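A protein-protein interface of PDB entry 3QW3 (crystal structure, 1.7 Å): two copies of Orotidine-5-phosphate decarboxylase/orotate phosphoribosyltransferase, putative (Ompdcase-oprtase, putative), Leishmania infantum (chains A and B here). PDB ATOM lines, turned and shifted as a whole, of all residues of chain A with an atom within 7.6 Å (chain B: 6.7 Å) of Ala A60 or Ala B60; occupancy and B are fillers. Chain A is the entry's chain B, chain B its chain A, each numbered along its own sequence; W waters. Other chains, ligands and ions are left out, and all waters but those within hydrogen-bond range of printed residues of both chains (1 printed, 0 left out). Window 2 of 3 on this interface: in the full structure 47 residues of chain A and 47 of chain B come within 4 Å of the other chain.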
ATOM      1  N   ALA A  27      -1.477 -30.035 -17.585  1.00  0.00           N
ATOM      2  CA  ALA A  27      -0.071 -30.452 -17.637  1.00  0.00           C
ATOM      3  C   ALA A  27       0.610 -30.396 -16.265  1.00  0.00           C
ATOM      4  O   ALA A  27       1.356 -31.309 -15.897  1.00  0.00           O
ATOM      5  CB  ALA A  27       0.702 -29.618 -18.656  1.00  0.00           C
ATOM      6  N   PHE A  55       0.813 -36.882 -23.032  1.00  0.00           N
ATOM      7  CA  PHE A  55       1.557 -35.640 -22.870  1.00  0.00           C
ATOM      8  C   PHE A  55       1.368 -34.673 -24.034  1.00  0.00           C
ATOM      9  O   PHE A  55       1.241 -33.470 -23.822  1.00  0.00           O
ATOM     10  CB  PHE A  55       3.028 -35.918 -22.580  1.00  0.00           C
ATOM     11  CG  PHE A  55       3.270 -36.398 -21.176  1.00  0.00           C
ATOM     12  CD1 PHE A  55       3.488 -35.481 -20.145  1.00  0.00           C
ATOM     13  CD2 PHE A  55       3.236 -37.759 -20.873  1.00  0.00           C
ATOM     14  CE1 PHE A  55       3.699 -35.918 -18.828  1.00  0.00           C
ATOM     15  CE2 PHE A  55       3.443 -38.205 -19.567  1.00  0.00           C
ATOM     16  CZ  PHE A  55       3.678 -37.281 -18.543  1.00  0.00           C
ATOM     17  N   GLU A  56       1.332 -35.205 -25.255  1.00  0.00           N
ATOM     18  CA  GLU A  56       1.044 -34.402 -26.447  1.00  0.00           C
ATOM     19  C   GLU A  56      -0.310 -33.699 -26.308  1.00  0.00           C
ATOM     20  O   GLU A  56      -0.462 -32.539 -26.704  1.00  0.00           O
ATOM     21  CB  GLU A  56       1.064 -35.280 -27.707  1.00  0.00           C
ATOM     22  CG  GLU A  56       0.796 -34.518 -29.013  1.00  0.00           C
ATOM     23  CD  GLU A  56       0.669 -35.421 -30.236  1.00  0.00           C
ATOM     24  OE1 GLU A  56      -0.226 -35.163 -31.069  1.00  0.00           O
ATOM     25  OE2 GLU A  56       1.458 -36.379 -30.377  1.00  0.00           O
ATOM     26  N   PHE A  57      -1.271 -34.420 -25.732  1.00  0.00           N
ATOM     27  CA  PHE A  57      -2.638 -33.942 -25.509  1.00  0.00           C
ATOM     28  C   PHE A  57      -2.686 -32.561 -24.841  1.00  0.00           C
ATOM     29  O   PHE A  57      -3.561 -31.750 -25.153  1.00  0.00           O
ATOM     30  CB  PHE A  57      -3.406 -34.979 -24.676  1.00  0.00           C
ATOM     31  CG  PHE A  57      -4.841 -34.616 -24.390  1.00  0.00           C
ATOM     32  CD1 PHE A  57      -5.173 -33.875 -23.262  1.00  0.00           C
ATOM     33  CD2 PHE A  57      -5.860 -35.055 -25.226  1.00  0.00           C
ATOM     34  CE1 PHE A  57      -6.497 -33.549 -22.982  1.00  0.00           C
ATOM     35  CE2 PHE A  57      -7.192 -34.737 -24.954  1.00  0.00           C
ATOM     36  CZ  PHE A  57      -7.507 -33.979 -23.830  1.00  0.00           C
ATOM     37  N   PHE A  58      -1.748 -32.294 -23.937  1.00  0.00           N
ATOM     38  CA  PHE A  58      -1.716 -31.012 -23.217  1.00  0.00           C
ATOM     39  C   PHE A  58      -1.173 -29.842 -24.048  1.00  0.00           C
ATOM     40  O   PHE A  58      -1.122 -28.704 -23.573  1.00  0.00           O
ATOM     41  CB  PHE A  58      -0.945 -31.139 -21.898  1.00  0.00           C
ATOM     42  CG  PHE A  58      -1.571 -32.092 -20.921  1.00  0.00           C
ATOM     43  CD1 PHE A  58      -2.817 -31.822 -20.362  1.00  0.00           C
ATOM     44  CD2 PHE A  58      -0.908 -33.253 -20.546  1.00  0.00           C
ATOM     45  CE1 PHE A  58      -3.400 -32.708 -19.458  1.00  0.00           C
ATOM     46  CE2 PHE A  58      -1.484 -34.142 -19.641  1.00  0.00           C
ATOM     47  CZ  PHE A  58      -2.731 -33.865 -19.099  1.00  0.00           C
ATOM     48  N   GLY A  59      -0.773 -30.127 -25.283  1.00  0.00           N
ATOM     49  CA  GLY A  59      -0.288 -29.104 -26.199  1.00  0.00           C
ATOM     50  C   GLY A  59       1.083 -28.570 -25.840  1.00  0.00           C
ATOM     51  O   GLY A  59       1.982 -29.332 -25.492  1.00  0.00           O
ATOM     52  N   ALA A  60       1.221 -27.249 -25.925  1.00  0.00           N
ATOM     53  CA  ALA A  60       2.471 -26.540 -25.645  1.00  0.00           C
ATOM     54  C   ALA A  60       3.150 -27.015 -24.360  1.00  0.00           C
ATOM     55  O   ALA A  60       4.300 -27.473 -24.383  1.00  0.00           O
ATOM     56  CB  ALA A  60       2.210 -25.029 -25.588  1.00  0.00           C
ATOM     57  N   GLU A  61       2.416 -26.944 -23.252  1.00  0.00           N
ATOM     58  CA  GLU A  61       2.950 -27.291 -21.933  1.00  0.00           C
ATOM     59  C   GLU A  61       3.192 -28.794 -21.776  1.00  0.00           C
ATOM     60  O   GLU A  61       3.903 -29.216 -20.861  1.00  0.00           O
ATOM     61  CB  GLU A  61       2.018 -26.796 -20.823  1.00  0.00           C
ATOM     62  CG  GLU A  61       1.883 -25.277 -20.747  1.00  0.00           C
ATOM     63  N   GLY A  62       2.599 -29.585 -22.669  1.00  0.00           N
ATOM     64  CA  GLY A  62       2.719 -31.047 -22.631  1.00  0.00           C
ATOM     65  C   GLY A  62       4.125 -31.585 -22.806  1.00  0.00           C
ATOM     66  O   GLY A  62       4.530 -32.528 -22.109  1.00  0.00           O
ATOM     67  N   TRP A  63       4.858 -31.009 -23.758  1.00  0.00           N
ATOM     68  CA  TRP A  63       6.259 -31.350 -23.971  1.00  0.00           C
ATOM     69  C   TRP A  63       7.086 -31.111 -22.713  1.00  0.00           C
ATOM     70  O   TRP A  63       7.839 -31.987 -22.278  1.00  0.00           O
ATOM     71  CB  TRP A  63       6.868 -30.516 -25.094  1.00  0.00           C
ATOM     72  CG  TRP A  63       8.325 -30.318 -24.854  1.00  0.00           C
ATOM     73  CD1 TRP A  63       8.903 -29.405 -24.020  1.00  0.00           C
ATOM     74  CD2 TRP A  63       9.390 -31.086 -25.402  1.00  0.00           C
ATOM     75  NE1 TRP A  63      10.263 -29.541 -24.033  1.00  0.00           N
ATOM     76  CE2 TRP A  63      10.591 -30.567 -24.877  1.00  0.00           C
ATOM     77  CE3 TRP A  63       9.451 -32.148 -26.303  1.00  0.00           C
ATOM     78  CZ2 TRP A  63      11.832 -31.076 -25.221  1.00  0.00           C
ATOM     79  CZ3 TRP A  63      10.681 -32.647 -26.642  1.00  0.00           C
ATOM     80  CH2 TRP A  63      11.857 -32.114 -26.101  1.00  0.00           C
ATOM     81  N   ALA A  64       6.939 -29.915 -22.143  1.00  0.00           N
ATOM     82  CA  ALA A  64       7.714 -29.494 -20.976  1.00  0.00           C
ATOM     83  C   ALA A  64       7.408 -30.416 -19.809  1.00  0.00           C
ATOM     84  O   ALA A  64       8.308 -30.802 -19.054  1.00  0.00           O
ATOM     85  CB  ALA A  64       7.391 -28.052 -20.613  1.00  0.00           C
ATOM     86  N   ALA A  65       6.131 -30.767 -19.689  1.00  0.00           N
ATOM     87  CA  ALA A  65       5.658 -31.693 -18.666  1.00  0.00           C
ATOM     88  C   ALA A  65       6.333 -33.050 -18.817  1.00  0.00           C
ATOM     89  O   ALA A  65       6.823 -33.614 -17.836  1.00  0.00           O
ATOM     90  CB  ALA A  65       4.143 -31.835 -18.741  1.00  0.00           C
ATOM     91  N   PHE B  55       8.382 -30.473 -36.127  1.00  0.00           N
ATOM     92  CA  PHE B  55       7.857 -29.551 -35.127  1.00  0.00           C
ATOM     93  C   PHE B  55       8.091 -30.049 -33.702  1.00  0.00           C
ATOM     94  O   PHE B  55       8.418 -29.260 -32.817  1.00  0.00           O
ATOM     95  CB  PHE B  55       6.388 -29.227 -35.395  1.00  0.00           C
ATOM     96  CG  PHE B  55       6.190 -28.320 -36.573  1.00  0.00           C
ATOM     97  CD1 PHE B  55       6.259 -26.935 -36.416  1.00  0.00           C
ATOM     98  CD2 PHE B  55       5.960 -28.843 -37.840  1.00  0.00           C
ATOM     99  CE1 PHE B  55       6.082 -26.082 -37.514  1.00  0.00           C
ATOM    100  CE2 PHE B  55       5.788 -27.998 -38.945  1.00  0.00           C
ATOM    101  CZ  PHE B  55       5.852 -26.617 -38.777  1.00  0.00           C
ATOM    102  N   GLU B  56       7.952 -31.359 -33.493  1.00  0.00           N
ATOM    103  CA  GLU B  56       8.264 -31.970 -32.200  1.00  0.00           C
ATOM    104  C   GLU B  56       9.717 -31.690 -31.796  1.00  0.00           C
ATOM    105  O   GLU B  56      10.013 -31.518 -30.610  1.00  0.00           O
ATOM    106  CB  GLU B  56       8.004 -33.484 -32.229  1.00  0.00           C
ATOM    107  CG  GLU B  56       8.291 -34.163 -30.886  1.00  0.00           C
ATOM    108  CD  GLU B  56       8.173 -35.674 -30.929  1.00  0.00           C
ATOM    109  OE1 GLU B  56       8.996 -36.347 -30.268  1.00  0.00           O
ATOM    110  OE2 GLU B  56       7.258 -36.193 -31.606  1.00  0.00           O
ATOM    111  N   PHE B  57      10.602 -31.634 -32.792  1.00  0.00           N
ATOM    112  CA  PHE B  57      12.038 -31.377 -32.600  1.00  0.00           C
ATOM    113  C   PHE B  57      12.305 -30.114 -31.774  1.00  0.00           C
ATOM    114  O   PHE B  57      13.231 -30.085 -30.959  1.00  0.00           O
ATOM    115  CB  PHE B  57      12.736 -31.283 -33.969  1.00  0.00           C
ATOM    116  CG  PHE B  57      14.229 -31.051 -33.899  1.00  0.00           C
ATOM    117  CD1 PHE B  57      14.746 -29.761 -33.786  1.00  0.00           C
ATOM    118  CD2 PHE B  57      15.114 -32.120 -33.991  1.00  0.00           C
ATOM    119  CE1 PHE B  57      16.127 -29.542 -33.731  1.00  0.00           C
ATOM    120  CE2 PHE B  57      16.496 -31.911 -33.947  1.00  0.00           C
ATOM    121  CZ  PHE B  57      17.000 -30.619 -33.815  1.00  0.00           C
ATOM    122  N   PHE B  58      11.490 -29.082 -31.973  1.00  0.00           N
ATOM    123  CA  PHE B  58      11.677 -27.814 -31.266  1.00  0.00           C
ATOM    124  C   PHE B  58      11.133 -27.795 -29.839  1.00  0.00           C
ATOM    125  O   PHE B  58      11.175 -26.762 -29.166  1.00  0.00           O
ATOM    126  CB  PHE B  58      11.118 -26.651 -32.088  1.00  0.00           C
ATOM    127  CG  PHE B  58      11.833 -26.451 -33.387  1.00  0.00           C
ATOM    128  CD1 PHE B  58      13.167 -26.044 -33.403  1.00  0.00           C
ATOM    129  CD2 PHE B  58      11.188 -26.682 -34.593  1.00  0.00           C
ATOM    130  CE1 PHE B  58      13.843 -25.873 -34.602  1.00  0.00           C
ATOM    131  CE2 PHE B  58      11.857 -26.505 -35.800  1.00  0.00           C
ATOM    132  CZ  PHE B  58      13.188 -26.099 -35.800  1.00  0.00           C
ATOM    133  N   GLY B  59      10.626 -28.937 -29.385  1.00  0.00           N
ATOM    134  CA  GLY B  59      10.200 -29.101 -27.999  1.00  0.00           C
ATOM    135  C   GLY B  59       8.970 -28.300 -27.631  1.00  0.00           C
ATOM    136  O   GLY B  59       7.969 -28.319 -28.350  1.00  0.00           O
ATOM    137  N   ALA B  60       9.057 -27.586 -26.511  1.00  0.00           N
ATOM    138  CA  ALA B  60       7.941 -26.788 -26.009  1.00  0.00           C
ATOM    139  C   ALA B  60       7.411 -25.866 -27.100  1.00  0.00           C
ATOM    140  O   ALA B  60       6.225 -25.918 -27.444  1.00  0.00           O
ATOM    141  CB  ALA B  60       8.366 -25.989 -24.782  1.00  0.00           C
ATOM    142  N   GLU B  61       8.305 -25.068 -27.676  1.00  0.00           N
ATOM    143  CA  GLU B  61       7.940 -24.104 -28.711  1.00  0.00           C
ATOM    144  C   GLU B  61       7.417 -24.772 -29.980  1.00  0.00           C
ATOM    145  O   GLU B  61       6.703 -24.151 -30.766  1.00  0.00           O
ATOM    146  CB  GLU B  61       9.135 -23.218 -29.051  1.00  0.00           C
ATOM    147  CG  GLU B  61       9.526 -22.250 -27.949  1.00  0.00           C
ATOM    148  CD  GLU B  61      10.394 -21.120 -28.461  1.00  0.00           C
ATOM    149  OE1 GLU B  61      11.485 -21.401 -29.005  1.00  0.00           O
ATOM    150  OE2 GLU B  61       9.985 -19.947 -28.316  1.00  0.00           O
ATOM    151  N   GLY B  62       7.773 -26.042 -30.161  1.00  0.00           N
ATOM    152  CA  GLY B  62       7.374 -26.816 -31.332  1.00  0.00           C
ATOM    153  C   GLY B  62       5.883 -26.987 -31.563  1.00  0.00           C
ATOM    154  O   GLY B  62       5.413 -26.813 -32.692  1.00  0.00           O
ATOM    155  N   TRP B  63       5.143 -27.355 -30.510  1.00  0.00           N
ATOM    156  CA  TRP B  63       3.684 -27.540 -30.600  1.00  0.00           C
ATOM    157  C   TRP B  63       3.000 -26.251 -31.008  1.00  0.00           C
ATOM    158  O   TRP B  63       2.142 -26.243 -31.894  1.00  0.00           O
ATOM    159  CB  TRP B  63       3.074 -28.011 -29.271  1.00  0.00           C
ATOM    160  CG  TRP B  63       1.571 -28.247 -29.360  1.00  0.00           C
ATOM    161  CD1 TRP B  63       0.945 -29.439 -29.585  1.00  0.00           C
ATOM    162  CD2 TRP B  63       0.524 -27.266 -29.243  1.00  0.00           C
ATOM    163  NE1 TRP B  63      -0.417 -29.266 -29.607  1.00  0.00           N
ATOM    164  CE2 TRP B  63      -0.701 -27.943 -29.402  1.00  0.00           C
ATOM    165  CE3 TRP B  63       0.506 -25.887 -29.013  1.00  0.00           C
ATOM    166  CZ2 TRP B  63      -1.933 -27.287 -29.339  1.00  0.00           C
ATOM    167  CZ3 TRP B  63      -0.717 -25.236 -28.953  1.00  0.00           C
ATOM    168  CH2 TRP B  63      -1.918 -25.937 -29.115  1.00  0.00           C
ATOM    169  N   ALA B  64       3.392 -25.162 -30.350  1.00  0.00           N
ATOM    170  CA  ALA B  64       2.799 -23.845 -30.600  1.00  0.00           C
ATOM    171  C   ALA B  64       3.101 -23.399 -32.029  1.00  0.00           C
ATOM    172  O   ALA B  64       2.250 -22.811 -32.692  1.00  0.00           O
ATOM    173  CB  ALA B  64       3.303 -22.817 -29.595  1.00  0.00           C
ATOM    174  N   ALA B  65       4.314 -23.704 -32.489  1.00  0.00           N
ATOM    175  CA  ALA B  65       4.733 -23.408 -33.854  1.00  0.00           C
ATOM    176  C   ALA B  65       3.878 -24.171 -34.866  1.00  0.00           C
ATOM    177  O   ALA B  65       3.433 -23.601 -35.864  1.00  0.00           O
ATOM    178  CB  ALA B  65       6.214 -23.732 -34.045  1.00  0.00           C
HETATM  179  O   HOH W   1      -2.392 -31.526 -28.397  1.00  0.00           O
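N of Ala B60 lies close to NE1 of Trp A63 (3.4 Å).
Among the printed residues, merely in contact across the chains: Trp A63 with Gly B59 (3.4 Å), Ala A60 with Trp B63 (3.4 Å), Gly A59 with Trp B63 (3.4 Å) and Ala A60 with Ala B60 (3.9 Å).
Of the printed residues of chain B, Ala A60 touches Ala B60 and Trp B63.
Printed residues of chain A within 4 Å of Ala B60: Ala A60 and Trp A63.
Of the printed residues of chain A, Trp B63 touches Gly A59 (3.4 Å) and Ala A60 (3.4 Å).
Of the printed residues of chain B, Trp A63 touches Gly B59 and Ala B60.
Of the printed residues of chain B, Gly A59 touches Trp B63.
Of the printed residues of chain A, Gly B59 touches Trp A63.
Glu A56 touches none of the printed residues of chain B.
Phe A57 touches none of the printed residues of chain B.
The nearest printed residue of chain B that does not touch Ala A60 is Ala B64 (4.7 Å).
The nearest printed residue of chain A that does not touch Ala B60 is Ala A64 (4.8 Å).
Of the 11 printed residues of chain B, 3 touch a printed residue of chain A.
Printed residues of chain B that touch a printed residue of chain A: Gly B59, Ala B60 and Trp B63.
Hydrophobic or aromatic side chains of chain B that line the printed part of chain A: Ala B60 and Trp B63.
Along chain B the printed residues that touch a printed residue of chain A span positions 59 to 63.
Of the 12 printed residues of chain A, 3 touch a printed residue of chain B.
Printed residues of chain A that touch a printed residue of chain B: Gly A59, Ala A60 and Trp A63.
Hydrophobic or aromatic side chains of chain A that line the printed part of chain B: Ala A60 and Trp A63.
Along chain A the printed residues that touch a printed residue of chain B span positions 59 to 63.
Gly A59 touches Trp B63, and with the chains exchanged Trp A63 touches Gly B59.
Ala A60 touches its own counterpart, Ala B60.
Ala A60 touches Trp B63, and with the chains exchanged Trp A63 touches Ala B60.
Positions printed for both chains: 55, 56, 57, 58, 59, 60, 61, 62, 63, 64 and 65.
Of the 5 pairs that touch across the chains among the printed residues, 5 have their exchanged pair printed and touching as well.
Water W1 lies within hydrogen-bond range of the backbone carbonyl oxygen (O) of Glu A56 (2.8 Å), the indole nitrogen (NE1) of Trp B63 (3.2 Å) and the backbone carbonyl oxygen (O) of Phe A57 (3.5 Å).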
